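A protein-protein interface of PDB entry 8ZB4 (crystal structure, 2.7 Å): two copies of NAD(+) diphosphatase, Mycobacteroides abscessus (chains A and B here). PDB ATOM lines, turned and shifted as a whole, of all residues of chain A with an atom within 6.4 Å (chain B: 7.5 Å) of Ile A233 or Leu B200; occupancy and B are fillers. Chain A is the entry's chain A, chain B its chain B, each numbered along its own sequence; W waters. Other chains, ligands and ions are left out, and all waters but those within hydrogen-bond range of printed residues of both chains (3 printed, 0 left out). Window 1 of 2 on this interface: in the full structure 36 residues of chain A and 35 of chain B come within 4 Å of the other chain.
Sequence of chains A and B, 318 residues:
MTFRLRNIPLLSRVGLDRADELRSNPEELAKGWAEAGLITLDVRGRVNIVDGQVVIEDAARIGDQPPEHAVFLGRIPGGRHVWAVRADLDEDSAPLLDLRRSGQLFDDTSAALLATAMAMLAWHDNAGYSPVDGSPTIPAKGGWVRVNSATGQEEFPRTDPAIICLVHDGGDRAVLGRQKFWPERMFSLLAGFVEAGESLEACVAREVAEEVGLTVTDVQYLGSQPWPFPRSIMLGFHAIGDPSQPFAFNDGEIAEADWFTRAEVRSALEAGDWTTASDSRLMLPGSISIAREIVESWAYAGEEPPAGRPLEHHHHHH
OE1 of Glu B201 lies within hydrogen-bond range of OH of Tyr A221 (2.5 Å). The side-chain hydroxyl (OG) of Ser A224 sits at hydrogen-bond distance from the backbone NH (N) of Leu B200 (3.1 Å). The side-chain hydroxyl (OG) of Ser A224 sits at hydrogen-bond distance from the side-chain carboxylate (OE2) of Glu B201 (2.7 Å).
The backbone carbonyl oxygen of Asp A160 sits at hydrogen-bond distance from the backbone NH of Ile A233 (3.0 Å). N of Ala A162 sits at hydrogen-bond distance from O of Ile A233 (3.0 Å). OG of Ser A224 lies within hydrogen-bond range of OH of Tyr A221, at 3.3 Å. The backbone NH (N) of Leu B235 lies within hydrogen-bond range of the backbone carbonyl oxygen (O) of Ala B162. SG of Cys B203 sits close to OE2 of Glu B198 (3.4 Å). N of Glu B201 sits close to OG of Ser B199, at 3.4 Å.
Among the printed residues, pairs that only touch across the chains: Tyr A221 with Tyr B221 (3.2 Å), Thr A159 with Pro B161 (3.3 Å), Ser A224 with Ser B199 (3.5 Å), Ile A233 with Glu B198 (3.6 Å), Leu A200 with Leu B235 (3.6 Å), Pro A226 with Gly B197 (3.7 Å), Leu A235 with Leu B200 (3.7 Å), Leu A200 with Tyr B221 (3.8 Å), Pro A226 with Glu B198 (3.8 Å), Ile A233 with Leu B200 (3.8 Å) and Tyr A221 with Leu B200 (3.9 Å).
Ala A162 touches none of the printed residues of chain B. Of the printed residues of chain B, Leu A200 touches Tyr B221 (3.8 Å) and Leu B235 (3.6 Å). Of the printed residues of chain B, Tyr A221 touches Leu B200, Glu B201 and Tyr B221. Gln A225 touches none of the printed residues of chain B. Printed residues of chain B within 4 Å of Pro A226: Gly B197 (3.7 Å) and Glu B198 (3.8 Å). Ile A233 touches just these residues of chain B: Glu B198 and Leu B200. Of the printed residues of chain A, Gly B197 touches Pro A226 (3.7 Å). Leu B200 touches just these residues of chain A: Tyr A221 (3.9 Å), Ser A224 (3.1 Å), Ile A233 (3.8 Å) and Leu A235 (3.7 Å). Printed residues of chain A within 4 Å of Tyr B221: Leu A200 (3.8 Å) and Tyr A221 (3.2 Å). The nearest residue of chain B that does not touch Ile A233 is Val B194 (4.2 Å). The nearest residue of chain A that does not touch Leu B200 is Leu A200 (5.7 Å).
Printed residues of chain B that touch a printed residue of chain A: Pro B161, Gly B197, Glu B198, Ser B199, Leu B200, Glu B201, Tyr B221 and Leu B235. Hydrophobic or aromatic side chains of chain B within 4 Å of the printed part of chain A: Pro B161, Leu B200, Tyr B221 and Leu B235. Along chain B the printed residues that touch a printed residue of chain A span positions 161 to 235. Of the 18 printed residues of chain A, 7 touch a printed residue of chain B. Printed residues of chain A that touch a printed residue of chain B: Thr A159, Leu A200, Tyr A221, Ser A224, Pro A226, Ile A233 and Leu A235. Along chain A the printed residues that touch a printed residue of chain B span positions 159 to 235.
Leu A200 touches Tyr B221, and with the chains exchanged Tyr A221 touches Leu B200. Leu A200 touches Leu B235, and with the chains exchanged Leu A235 touches Leu B200. Tyr B221 touches its own counterpart, Tyr A221. Positions printed for both chains: 161, 162, 163, 200, 221 and 235.
Water W2 lies within hydrogen-bond range of OG1 of Thr A159 (2.6 Å) and O of Val B194 (2.8 Å). Water W1 bridges the backbone NH of Gly B197 and the backbone carbonyl oxygen of Ser A232. Water W3 bridges OE2 of Glu B201 (3.0 Å) and N of Ser A224 (3.1 Å).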
ATOM      1  N   THR A 159     -19.769  14.941 -36.666  1.00  0.00           N
ATOM      2  CA  THR A 159     -19.929  13.854 -35.713  1.00  0.00           C
ATOM      3  C   THR A 159     -21.382  13.815 -35.237  1.00  0.00           C
ATOM      4  O   THR A 159     -21.858  14.788 -34.678  1.00  0.00           O
ATOM      5  CB  THR A 159     -18.941  14.091 -34.575  1.00  0.00           C
ATOM      6  OG1 THR A 159     -17.649  14.078 -35.177  1.00  0.00           O
ATOM      7  CG2 THR A 159     -18.952  12.994 -33.527  1.00  0.00           C
ATOM      8  N   ASP A 160     -22.091  12.709 -35.499  1.00  0.00           N
ATOM      9  CA  ASP A 160     -23.501  12.553 -35.169  1.00  0.00           C
ATOM     10  C   ASP A 160     -23.650  11.957 -33.769  1.00  0.00           C
ATOM     11  O   ASP A 160     -23.161  10.866 -33.500  1.00  0.00           O
ATOM     12  CB  ASP A 160     -24.216  11.625 -36.144  1.00  0.00           C
ATOM     13  CG  ASP A 160     -24.374  12.141 -37.568  1.00  0.00           C
ATOM     14  OD1 ASP A 160     -24.135  13.346 -37.781  1.00  0.00           O
ATOM     15  OD2 ASP A 160     -24.708  11.329 -38.470  1.00  0.00           O
ATOM     16  N   PRO A 161     -24.346  12.617 -32.828  1.00  0.00           N
ATOM     17  CA  PRO A 161     -24.483  12.081 -31.475  1.00  0.00           C
ATOM     18  C   PRO A 161     -25.587  11.035 -31.397  1.00  0.00           C
ATOM     19  O   PRO A 161     -26.617  11.186 -32.046  1.00  0.00           O
ATOM     20  CB  PRO A 161     -24.819  13.326 -30.683  1.00  0.00           C
ATOM     21  CG  PRO A 161     -25.668  14.108 -31.647  1.00  0.00           C
ATOM     22  CD  PRO A 161     -25.010  13.911 -32.999  1.00  0.00           C
ATOM     23  N   ALA A 162     -25.352   9.998 -30.581  1.00  0.00           N
ATOM     24  CA  ALA A 162     -26.298   8.910 -30.376  1.00  0.00           C
ATOM     25  C   ALA A 162     -26.261   8.466 -28.913  1.00  0.00           C
ATOM     26  O   ALA A 162     -25.205   8.476 -28.285  1.00  0.00           O
ATOM     27  CB  ALA A 162     -25.963   7.757 -31.304  1.00  0.00           C
ATOM     28  N   ILE A 163     -27.416   8.076 -28.367  1.00  0.00           N
ATOM     29  CA  ILE A 163     -27.461   7.649 -26.976  1.00  0.00           C
ATOM     30  C   ILE A 163     -27.462   6.127 -26.936  1.00  0.00           C
ATOM     31  O   ILE A 163     -27.909   5.489 -27.884  1.00  0.00           O
ATOM     32  CB  ILE A 163     -28.653   8.254 -26.205  1.00  0.00           C
ATOM     33  CG1 ILE A 163     -30.009   7.816 -26.761  1.00  0.00           C
ATOM     34  CG2 ILE A 163     -28.535   9.774 -26.148  1.00  0.00           C
ATOM     35  CD1 ILE A 163     -30.466   6.445 -26.288  1.00  0.00           C
ATOM     36  N   LEU A 200     -30.579  15.287 -24.840  1.00  0.00           N
ATOM     37  CA  LEU A 200     -30.169  13.906 -24.656  1.00  0.00           C
ATOM     38  C   LEU A 200     -31.192  13.178 -23.782  1.00  0.00           C
ATOM     39  O   LEU A 200     -31.598  12.054 -24.098  1.00  0.00           O
ATOM     40  CB  LEU A 200     -28.764  13.831 -24.055  1.00  0.00           C
ATOM     41  CG  LEU A 200     -27.614  14.439 -24.865  1.00  0.00           C
ATOM     42  CD1 LEU A 200     -26.298  14.144 -24.181  1.00  0.00           C
ATOM     43  CD2 LEU A 200     -27.537  13.950 -26.304  1.00  0.00           C
ATOM     44  N   TYR A 221     -26.218  10.382 -17.279  1.00  0.00           N
ATOM     45  CA  TYR A 221     -24.993  10.183 -18.032  1.00  0.00           C
ATOM     46  C   TYR A 221     -23.955   9.369 -17.265  1.00  0.00           C
ATOM     47  O   TYR A 221     -23.684   9.647 -16.099  1.00  0.00           O
ATOM     48  CB  TYR A 221     -24.376  11.559 -18.288  1.00  0.00           C
ATOM     49  CG  TYR A 221     -23.099  11.586 -19.115  1.00  0.00           C
ATOM     50  CD1 TYR A 221     -23.134  11.403 -20.493  1.00  0.00           C
ATOM     51  CD2 TYR A 221     -21.876  11.877 -18.533  1.00  0.00           C
ATOM     52  CE1 TYR A 221     -21.983  11.466 -21.258  1.00  0.00           C
ATOM     53  CE2 TYR A 221     -20.716  11.942 -19.285  1.00  0.00           C
ATOM     54  CZ  TYR A 221     -20.772  11.739 -20.653  1.00  0.00           C
ATOM     55  OH  TYR A 221     -19.621  11.801 -21.379  1.00  0.00           O
ATOM     56  N   GLY A 223     -20.945   8.110 -19.471  1.00  0.00           N
ATOM     57  CA  GLY A 223     -19.748   8.488 -20.205  1.00  0.00           C
ATOM     58  C   GLY A 223     -19.986   8.542 -21.712  1.00  0.00           C
ATOM     59  O   GLY A 223     -21.126   8.485 -22.174  1.00  0.00           O
ATOM     60  N   SER A 224     -18.882   8.629 -22.462  1.00  0.00           N
ATOM     61  CA  SER A 224     -18.917   8.861 -23.896  1.00  0.00           C
ATOM     62  C   SER A 224     -17.746   8.172 -24.583  1.00  0.00           C
ATOM     63  O   SER A 224     -16.687   7.985 -23.991  1.00  0.00           O
ATOM     64  CB  SER A 224     -18.881  10.326 -24.205  1.00  0.00           C
ATOM     65  OG  SER A 224     -17.644  10.900 -23.797  1.00  0.00           O
ATOM     66  N   GLN A 225     -17.932   7.893 -25.879  1.00  0.00           N
ATOM     67  CA  GLN A 225     -16.973   7.137 -26.665  1.00  0.00           C
ATOM     68  C   GLN A 225     -17.060   7.541 -28.135  1.00  0.00           C
ATOM     69  O   GLN A 225     -18.128   7.440 -28.738  1.00  0.00           O
ATOM     70  CB  GLN A 225     -17.362   5.669 -26.504  1.00  0.00           C
ATOM     71  CG  GLN A 225     -16.475   4.703 -27.276  1.00  0.00           C
ATOM     72  CD  GLN A 225     -16.976   3.276 -27.265  1.00  0.00           C
ATOM     73  OE1 GLN A 225     -16.207   2.346 -27.010  1.00  0.00           O
ATOM     74  NE2 GLN A 225     -18.251   3.077 -27.562  1.00  0.00           N
ATOM     75  N   PRO A 226     -15.936   7.939 -28.777  1.00  0.00           N
ATOM     76  CA  PRO A 226     -15.910   8.182 -30.218  1.00  0.00           C
ATOM     77  C   PRO A 226     -16.261   6.877 -30.917  1.00  0.00           C
ATOM     78  O   PRO A 226     -15.832   5.831 -30.447  1.00  0.00           O
ATOM     79  CB  PRO A 226     -14.497   8.667 -30.558  1.00  0.00           C
ATOM     80  CG  PRO A 226     -13.680   8.379 -29.334  1.00  0.00           C
ATOM     81  CD  PRO A 226     -14.631   8.174 -28.156  1.00  0.00           C
ATOM     82  N   TRP A 227     -17.049   6.950 -32.006  1.00  0.00           N
ATOM     83  CA  TRP A 227     -17.545   5.750 -32.668  1.00  0.00           C
ATOM     84  C   TRP A 227     -17.544   5.913 -34.190  1.00  0.00           C
ATOM     85  O   TRP A 227     -18.599   5.940 -34.824  1.00  0.00           O
ATOM     86  CB  TRP A 227     -18.938   5.396 -32.134  1.00  0.00           C
ATOM     87  CG  TRP A 227     -19.340   3.970 -32.392  1.00  0.00           C
ATOM     88  CD1 TRP A 227     -20.325   3.522 -33.222  1.00  0.00           C
ATOM     89  CD2 TRP A 227     -18.750   2.793 -31.800  1.00  0.00           C
ATOM     90  NE1 TRP A 227     -20.392   2.153 -33.193  1.00  0.00           N
ATOM     91  CE2 TRP A 227     -19.436   1.678 -32.330  1.00  0.00           C
ATOM     92  CE3 TRP A 227     -17.713   2.575 -30.886  1.00  0.00           C
ATOM     93  CZ2 TRP A 227     -19.118   0.372 -31.967  1.00  0.00           C
ATOM     94  CZ3 TRP A 227     -17.382   1.283 -30.541  1.00  0.00           C
ATOM     95  CH2 TRP A 227     -18.088   0.199 -31.068  1.00  0.00           C
ATOM     96  N   PRO A 228     -16.349   5.962 -34.827  1.00  0.00           N
ATOM     97  CA  PRO A 228     -16.238   6.313 -36.247  1.00  0.00           C
ATOM     98  C   PRO A 228     -16.625   5.237 -37.262  1.00  0.00           C
ATOM     99  O   PRO A 228     -15.850   4.894 -38.152  1.00  0.00           O
ATOM    100  CB  PRO A 228     -14.757   6.711 -36.369  1.00  0.00           C
ATOM    101  CG  PRO A 228     -14.061   5.837 -35.342  1.00  0.00           C
ATOM    102  CD  PRO A 228     -15.045   5.763 -34.171  1.00  0.00           C
ATOM    103  N   ARG A 231     -19.279   7.784 -38.365  1.00  0.00           N
ATOM    104  CA  ARG A 231     -19.095   9.134 -37.839  1.00  0.00           C
ATOM    105  C   ARG A 231     -19.922   9.441 -36.586  1.00  0.00           C
ATOM    106  O   ARG A 231     -20.440  10.542 -36.467  1.00  0.00           O
ATOM    107  CB  ARG A 231     -19.478  10.118 -38.955  1.00  0.00           C
ATOM    108  CG  ARG A 231     -20.949  10.005 -39.328  1.00  0.00           C
ATOM    109  CD  ARG A 231     -21.334  11.019 -40.359  1.00  0.00           C
ATOM    110  NE  ARG A 231     -22.785  11.029 -40.581  1.00  0.00           N
ATOM    111  CZ  ARG A 231     -23.344  11.521 -41.690  1.00  0.00           C
ATOM    112  NH1 ARG A 231     -22.569  11.993 -42.650  1.00  0.00           N
ATOM    113  NH2 ARG A 231     -24.660  11.521 -41.842  1.00  0.00           N
ATOM    114  N   SER A 232     -20.024   8.510 -35.635  1.00  0.00           N
ATOM    115  CA  SER A 232     -20.863   8.724 -34.465  1.00  0.00           C
ATOM    116  C   SER A 232     -20.023   9.111 -33.249  1.00  0.00           C
ATOM    117  O   SER A 232     -18.802   8.974 -33.246  1.00  0.00           O
ATOM    118  CB  SER A 232     -21.703   7.513 -34.167  1.00  0.00           C
ATOM    119  OG  SER A 232     -22.742   7.366 -35.120  1.00  0.00           O
ATOM    120  N   ILE A 233     -20.702   9.630 -32.222  1.00  0.00           N
ATOM    121  CA  ILE A 233     -20.202   9.600 -30.857  1.00  0.00           C
ATOM    122  C   ILE A 233     -21.315   9.014 -30.006  1.00  0.00           C
ATOM    123  O   ILE A 233     -22.464   9.430 -30.139  1.00  0.00           O
ATOM    124  CB  ILE A 233     -19.755  10.978 -30.332  1.00  0.00           C
ATOM    125  CG1 ILE A 233     -19.238  10.862 -28.905  1.00  0.00           C
ATOM    126  CG2 ILE A 233     -20.865  12.025 -30.427  1.00  0.00           C
ATOM    127  CD1 ILE A 233     -18.498  12.087 -28.408  1.00  0.00           C
ATOM    128  N   MET A 234     -20.967   8.026 -29.175  1.00  0.00           N
ATOM    129  CA  MET A 234     -21.941   7.319 -28.360  1.00  0.00           C
ATOM    130  C   MET A 234     -21.919   7.892 -26.951  1.00  0.00           C
ATOM    131  O   MET A 234     -20.844   8.053 -26.382  1.00  0.00           O
ATOM    132  CB  MET A 234     -21.602   5.829 -28.272  1.00  0.00           C
ATOM    133  CG  MET A 234     -21.623   5.134 -29.593  1.00  0.00           C
ATOM    134  SD  MET A 234     -23.291   5.062 -30.271  1.00  0.00           S
ATOM    135  CE  MET A 234     -24.217   4.403 -28.880  1.00  0.00           C
ATOM    136  N   LEU A 235     -23.113   8.173 -26.412  1.00  0.00           N
ATOM    137  CA  LEU A 235     -23.253   8.810 -25.117  1.00  0.00           C
ATOM    138  C   LEU A 235     -24.047   7.889 -24.199  1.00  0.00           C
ATOM    139  O   LEU A 235     -25.221   7.612 -24.447  1.00  0.00           O
ATOM    140  CB  LEU A 235     -23.942  10.150 -25.346  1.00  0.00           C
ATOM    141  CG  LEU A 235     -23.297  11.043 -26.411  1.00  0.00           C
ATOM    142  CD1 LEU A 235     -24.096  12.317 -26.570  1.00  0.00           C
ATOM    143  CD2 LEU A 235     -21.859  11.384 -26.084  1.00  0.00           C
ATOM    144  N   PRO B 161     -22.634  18.517 -31.979  1.00  0.00           N
ATOM    145  CA  PRO B 161     -22.523  18.556 -30.524  1.00  0.00           C
ATOM    146  C   PRO B 161     -21.431  19.536 -30.106  1.00  0.00           C
ATOM    147  O   PRO B 161     -20.396  19.603 -30.759  1.00  0.00           O
ATOM    148  CB  PRO B 161     -22.196  17.115 -30.147  1.00  0.00           C
ATOM    149  CG  PRO B 161     -22.108  16.349 -31.475  1.00  0.00           C
ATOM    150  CD  PRO B 161     -21.937  17.373 -32.579  1.00  0.00           C
ATOM    151  N   ALA B 162     -21.693  20.286 -29.025  1.00  0.00           N
ATOM    152  CA  ALA B 162     -20.755  21.249 -28.478  1.00  0.00           C
ATOM    153  C   ALA B 162     -20.779  21.170 -26.954  1.00  0.00           C
ATOM    154  O   ALA B 162     -21.828  20.938 -26.352  1.00  0.00           O
ATOM    155  CB  ALA B 162     -21.102  22.639 -28.957  1.00  0.00           C
ATOM    156  N   ILE B 163     -19.616  21.369 -26.330  1.00  0.00           N
ATOM    157  CA  ILE B 163     -19.559  21.381 -24.878  1.00  0.00           C
ATOM    158  C   ILE B 163     -19.582  22.831 -24.408  1.00  0.00           C
ATOM    159  O   ILE B 163     -19.176  23.728 -25.149  1.00  0.00           O
ATOM    160  CB  ILE B 163     -18.338  20.605 -24.344  1.00  0.00           C
ATOM    161  CG1 ILE B 163     -16.988  21.220 -24.747  1.00  0.00           C
ATOM    162  CG2 ILE B 163     -18.418  19.139 -24.765  1.00  0.00           C
ATOM    163  CD1 ILE B 163     -16.569  22.437 -23.946  1.00  0.00           C
ATOM    164  N   VAL B 194     -17.313  19.533 -30.517  1.00  0.00           N
ATOM    165  CA  VAL B 194     -16.698  18.216 -30.442  1.00  0.00           C
ATOM    166  C   VAL B 194     -16.079  17.851 -31.792  1.00  0.00           C
ATOM    167  O   VAL B 194     -16.762  17.806 -32.811  1.00  0.00           O
ATOM    168  CB  VAL B 194     -17.747  17.162 -30.042  1.00  0.00           C
ATOM    169  CG1 VAL B 194     -17.157  15.759 -30.014  1.00  0.00           C
ATOM    170  CG2 VAL B 194     -18.403  17.490 -28.706  1.00  0.00           C
ATOM    171  N   GLU B 195     -14.783  17.561 -31.781  1.00  0.00           N
ATOM    172  CA  GLU B 195     -14.088  17.079 -32.963  1.00  0.00           C
ATOM    173  C   GLU B 195     -14.275  15.570 -33.099  1.00  0.00           C
ATOM    174  O   GLU B 195     -14.659  14.906 -32.135  1.00  0.00           O
ATOM    175  CB  GLU B 195     -12.612  17.452 -32.855  1.00  0.00           C
ATOM    176  CG  GLU B 195     -12.402  18.956 -32.973  1.00  0.00           C
ATOM    177  CD  GLU B 195     -10.959  19.416 -33.018  1.00  0.00           C
ATOM    178  OE1 GLU B 195     -10.752  20.647 -33.109  1.00  0.00           O
ATOM    179  OE2 GLU B 195     -10.041  18.567 -32.965  1.00  0.00           O
ATOM    180  N   GLY B 197     -13.226  11.774 -33.214  1.00  0.00           N
ATOM    181  CA  GLY B 197     -12.253  10.907 -32.565  1.00  0.00           C
ATOM    182  C   GLY B 197     -11.955  11.280 -31.111  1.00  0.00           C
ATOM    183  O   GLY B 197     -10.957  10.825 -30.563  1.00  0.00           O
ATOM    184  N   GLU B 198     -12.808  12.090 -30.472  1.00  0.00           N
ATOM    185  CA  GLU B 198     -12.591  12.420 -29.070  1.00  0.00           C
ATOM    186  C   GLU B 198     -13.877  12.230 -28.269  1.00  0.00           C
ATOM    187  O   GLU B 198     -14.974  12.337 -28.805  1.00  0.00           O
ATOM    188  CB  GLU B 198     -12.002  13.821 -28.908  1.00  0.00           C
ATOM    189  CG  GLU B 198     -12.991  14.938 -29.232  1.00  0.00           C
ATOM    190  CD  GLU B 198     -12.425  16.333 -29.066  1.00  0.00           C
ATOM    191  OE1 GLU B 198     -11.248  16.486 -28.656  1.00  0.00           O
ATOM    192  OE2 GLU B 198     -13.193  17.274 -29.356  1.00  0.00           O
ATOM    193  N   SER B 199     -13.702  11.908 -26.982  1.00  0.00           N
ATOM    194  CA  SER B 199     -14.788  11.855 -26.020  1.00  0.00           C
ATOM    195  C   SER B 199     -15.178  13.279 -25.638  1.00  0.00           C
ATOM    196  O   SER B 199     -14.370  14.194 -25.817  1.00  0.00           O
ATOM    197  CB  SER B 199     -14.350  11.101 -24.812  1.00  0.00           C
ATOM    198  OG  SER B 199     -13.371  11.873 -24.124  1.00  0.00           O
ATOM    199  N   LEU B 200     -16.384  13.449 -25.072  1.00  0.00           N
ATOM    200  CA  LEU B 200     -16.791  14.730 -24.511  1.00  0.00           C
ATOM    201  C   LEU B 200     -15.776  15.188 -23.458  1.00  0.00           C
ATOM    202  O   LEU B 200     -15.375  16.352 -23.456  1.00  0.00           O
ATOM    203  CB  LEU B 200     -18.203  14.662 -23.929  1.00  0.00           C
ATOM    204  CG  LEU B 200     -19.328  14.258 -24.895  1.00  0.00           C
ATOM    205  CD1 LEU B 200     -20.642  14.326 -24.126  1.00  0.00           C
ATOM    206  CD2 LEU B 200     -19.399  15.089 -26.178  1.00  0.00           C
ATOM    207  N   GLU B 201     -15.326  14.261 -22.601  1.00  0.00           N
ATOM    208  CA  GLU B 201     -14.428  14.597 -21.500  1.00  0.00           C
ATOM    209  C   GLU B 201     -13.096  15.144 -22.028  1.00  0.00           C
ATOM    210  O   GLU B 201     -12.533  16.091 -21.474  1.00  0.00           O
ATOM    211  CB  GLU B 201     -14.176  13.413 -20.563  1.00  0.00           C
ATOM    212  CG  GLU B 201     -15.397  12.938 -19.775  1.00  0.00           C
ATOM    213  CD  GLU B 201     -16.433  12.185 -20.592  1.00  0.00           C
ATOM    214  OE1 GLU B 201     -17.506  11.846 -20.057  1.00  0.00           O
ATOM    215  OE2 GLU B 201     -16.162  11.936 -21.784  1.00  0.00           O
ATOM    216  N   ALA B 202     -12.582  14.532 -23.101  1.00  0.00           N
ATOM    217  CA  ALA B 202     -11.380  15.010 -23.766  1.00  0.00           C
ATOM    218  C   ALA B 202     -11.628  16.355 -24.458  1.00  0.00           C
ATOM    219  O   ALA B 202     -10.768  17.238 -24.453  1.00  0.00           O
ATOM    220  CB  ALA B 202     -10.923  13.962 -24.754  1.00  0.00           C
ATOM    221  N   CYS B 203     -12.810  16.497 -25.067  1.00  0.00           N
ATOM    222  CA  CYS B 203     -13.186  17.734 -25.733  1.00  0.00           C
ATOM    223  C   CYS B 203     -13.210  18.905 -24.752  1.00  0.00           C
ATOM    224  O   CYS B 203     -12.744  19.991 -25.088  1.00  0.00           O
ATOM    225  CB  CYS B 203     -14.540  17.595 -26.414  1.00  0.00           C
ATOM    226  SG  CYS B 203     -15.129  19.122 -27.187  1.00  0.00           S
ATOM    227  N   VAL B 204     -13.748  18.689 -23.546  1.00  0.00           N
ATOM    228  CA  VAL B 204     -13.778  19.739 -22.535  1.00  0.00           C
ATOM    229  C   VAL B 204     -12.350  20.149 -22.181  1.00  0.00           C
ATOM    230  O   VAL B 204     -12.017  21.330 -22.268  1.00  0.00           O
ATOM    231  CB  VAL B 204     -14.561  19.361 -21.264  1.00  0.00           C
ATOM    232  CG1 VAL B 204     -14.423  20.419 -20.179  1.00  0.00           C
ATOM    233  CG2 VAL B 204     -16.035  19.123 -21.556  1.00  0.00           C
ATOM    234  N   ALA B 205     -11.515  19.175 -21.784  1.00  0.00           N
ATOM    235  CA  ALA B 205     -10.139  19.444 -21.383  1.00  0.00           C
ATOM    236  C   ALA B 205      -9.365  20.135 -22.503  1.00  0.00           C
ATOM    237  O   ALA B 205      -8.593  21.057 -22.243  1.00  0.00           O
ATOM    238  CB  ALA B 205      -9.459  18.170 -20.962  1.00  0.00           C
ATOM    239  N   ARG B 206      -9.587  19.695 -23.751  1.00  0.00           N
ATOM    240  CA  ARG B 206      -8.908  20.285 -24.893  1.00  0.00           C
ATOM    241  C   ARG B 206      -9.350  21.733 -25.096  1.00  0.00           C
ATOM    242  O   ARG B 206      -8.499  22.613 -25.173  1.00  0.00           O
ATOM    243  CB  ARG B 206      -9.122  19.473 -26.169  1.00  0.00           C
ATOM    244  CG  ARG B 206      -8.489  20.098 -27.408  1.00  0.00           C
ATOM    245  CD  ARG B 206      -8.737  19.275 -28.676  1.00  0.00           C
ATOM    246  NE  ARG B 206     -10.160  19.058 -28.957  1.00  0.00           N
ATOM    247  CZ  ARG B 206     -11.026  20.017 -29.264  1.00  0.00           C
ATOM    248  NH1 ARG B 206     -10.628  21.273 -29.367  1.00  0.00           N
ATOM    249  NH2 ARG B 206     -12.291  19.721 -29.492  1.00  0.00           N
ATOM    250  N   VAL B 219     -13.960  16.137 -14.874  1.00  0.00           N
ATOM    251  CA  VAL B 219     -14.917  16.681 -15.820  1.00  0.00           C
ATOM    252  C   VAL B 219     -16.236  15.945 -15.643  1.00  0.00           C
ATOM    253  O   VAL B 219     -16.269  14.736 -15.834  1.00  0.00           O
ATOM    254  CB  VAL B 219     -14.374  16.520 -17.253  1.00  0.00           C
ATOM    255  CG1 VAL B 219     -15.432  16.815 -18.306  1.00  0.00           C
ATOM    256  CG2 VAL B 219     -13.143  17.386 -17.488  1.00  0.00           C
ATOM    257  N   TYR B 221     -20.569  15.923 -16.389  1.00  0.00           N
ATOM    258  CA  TYR B 221     -21.783  16.322 -17.088  1.00  0.00           C
ATOM    259  C   TYR B 221     -22.841  16.846 -16.121  1.00  0.00           C
ATOM    260  O   TYR B 221     -23.093  16.236 -15.083  1.00  0.00           O
ATOM    261  CB  TYR B 221     -22.344  15.076 -17.778  1.00  0.00           C
ATOM    262  CG  TYR B 221     -23.632  15.253 -18.571  1.00  0.00           C
ATOM    263  CD1 TYR B 221     -23.621  15.850 -19.829  1.00  0.00           C
ATOM    264  CD2 TYR B 221     -24.842  14.755 -18.100  1.00  0.00           C
ATOM    265  CE1 TYR B 221     -24.782  15.977 -20.579  1.00  0.00           C
ATOM    266  CE2 TYR B 221     -26.008  14.872 -18.839  1.00  0.00           C
ATOM    267  CZ  TYR B 221     -25.979  15.487 -20.081  1.00  0.00           C
ATOM    268  OH  TYR B 221     -27.130  15.618 -20.809  1.00  0.00           O
ATOM    269  N   LEU B 235     -23.892  20.603 -24.475  1.00  0.00           N
ATOM    270  CA  LEU B 235     -23.711  19.628 -23.415  1.00  0.00           C
ATOM    271  C   LEU B 235     -22.926  20.286 -22.284  1.00  0.00           C
ATOM    272  O   LEU B 235     -21.759  20.645 -22.457  1.00  0.00           O
ATOM    273  CB  LEU B 235     -22.993  18.423 -24.018  1.00  0.00           C
ATOM    274  CG  LEU B 235     -23.619  17.877 -25.305  1.00  0.00           C
ATOM    275  CD1 LEU B 235     -22.758  16.793 -25.907  1.00  0.00           C
ATOM    276  CD2 LEU B 235     -25.037  17.379 -25.037  1.00  0.00           C
ATOM    277  N   GLY B 236     -23.599  20.450 -21.134  1.00  0.00           N
ATOM    278  CA  GLY B 236     -23.080  21.229 -20.024  1.00  0.00           C
ATOM    279  C   GLY B 236     -22.183  20.391 -19.117  1.00  0.00           C
ATOM    280  O   GLY B 236     -22.529  19.265 -18.762  1.00  0.00           O
ATOM    281  N   PHE B 237     -21.038  20.972 -18.737  1.00  0.00           N
ATOM    282  CA  PHE B 237     -20.072  20.320 -17.864  1.00  0.00           C
ATOM    283  C   PHE B 237     -19.527  21.314 -16.840  1.00  0.00           C
ATOM    284  O   PHE B 237     -19.543  22.522 -17.078  1.00  0.00           O
ATOM    285  CB  PHE B 237     -18.910  19.780 -18.708  1.00  0.00           C
ATOM    286  CG  PHE B 237     -19.233  18.523 -19.501  1.00  0.00           C
ATOM    287  CD1 PHE B 237     -19.118  17.267 -18.915  1.00  0.00           C
ATOM    288  CD2 PHE B 237     -19.665  18.595 -20.820  1.00  0.00           C
ATOM    289  CE1 PHE B 237     -19.442  16.119 -19.616  1.00  0.00           C
ATOM    290  CE2 PHE B 237     -19.968  17.442 -21.522  1.00  0.00           C
ATOM    291  CZ  PHE B 237     -19.854  16.204 -20.923  1.00  0.00           C
HETATM  292  O   HOH W   1     -15.678  10.374 -33.111  1.00  0.00           O
HETATM  293  O   HOH W   2     -16.937  16.594 -35.352  1.00  0.00           O
HETATM  294  O   HOH W   3     -16.198   9.077 -20.952  1.00  0.00           O
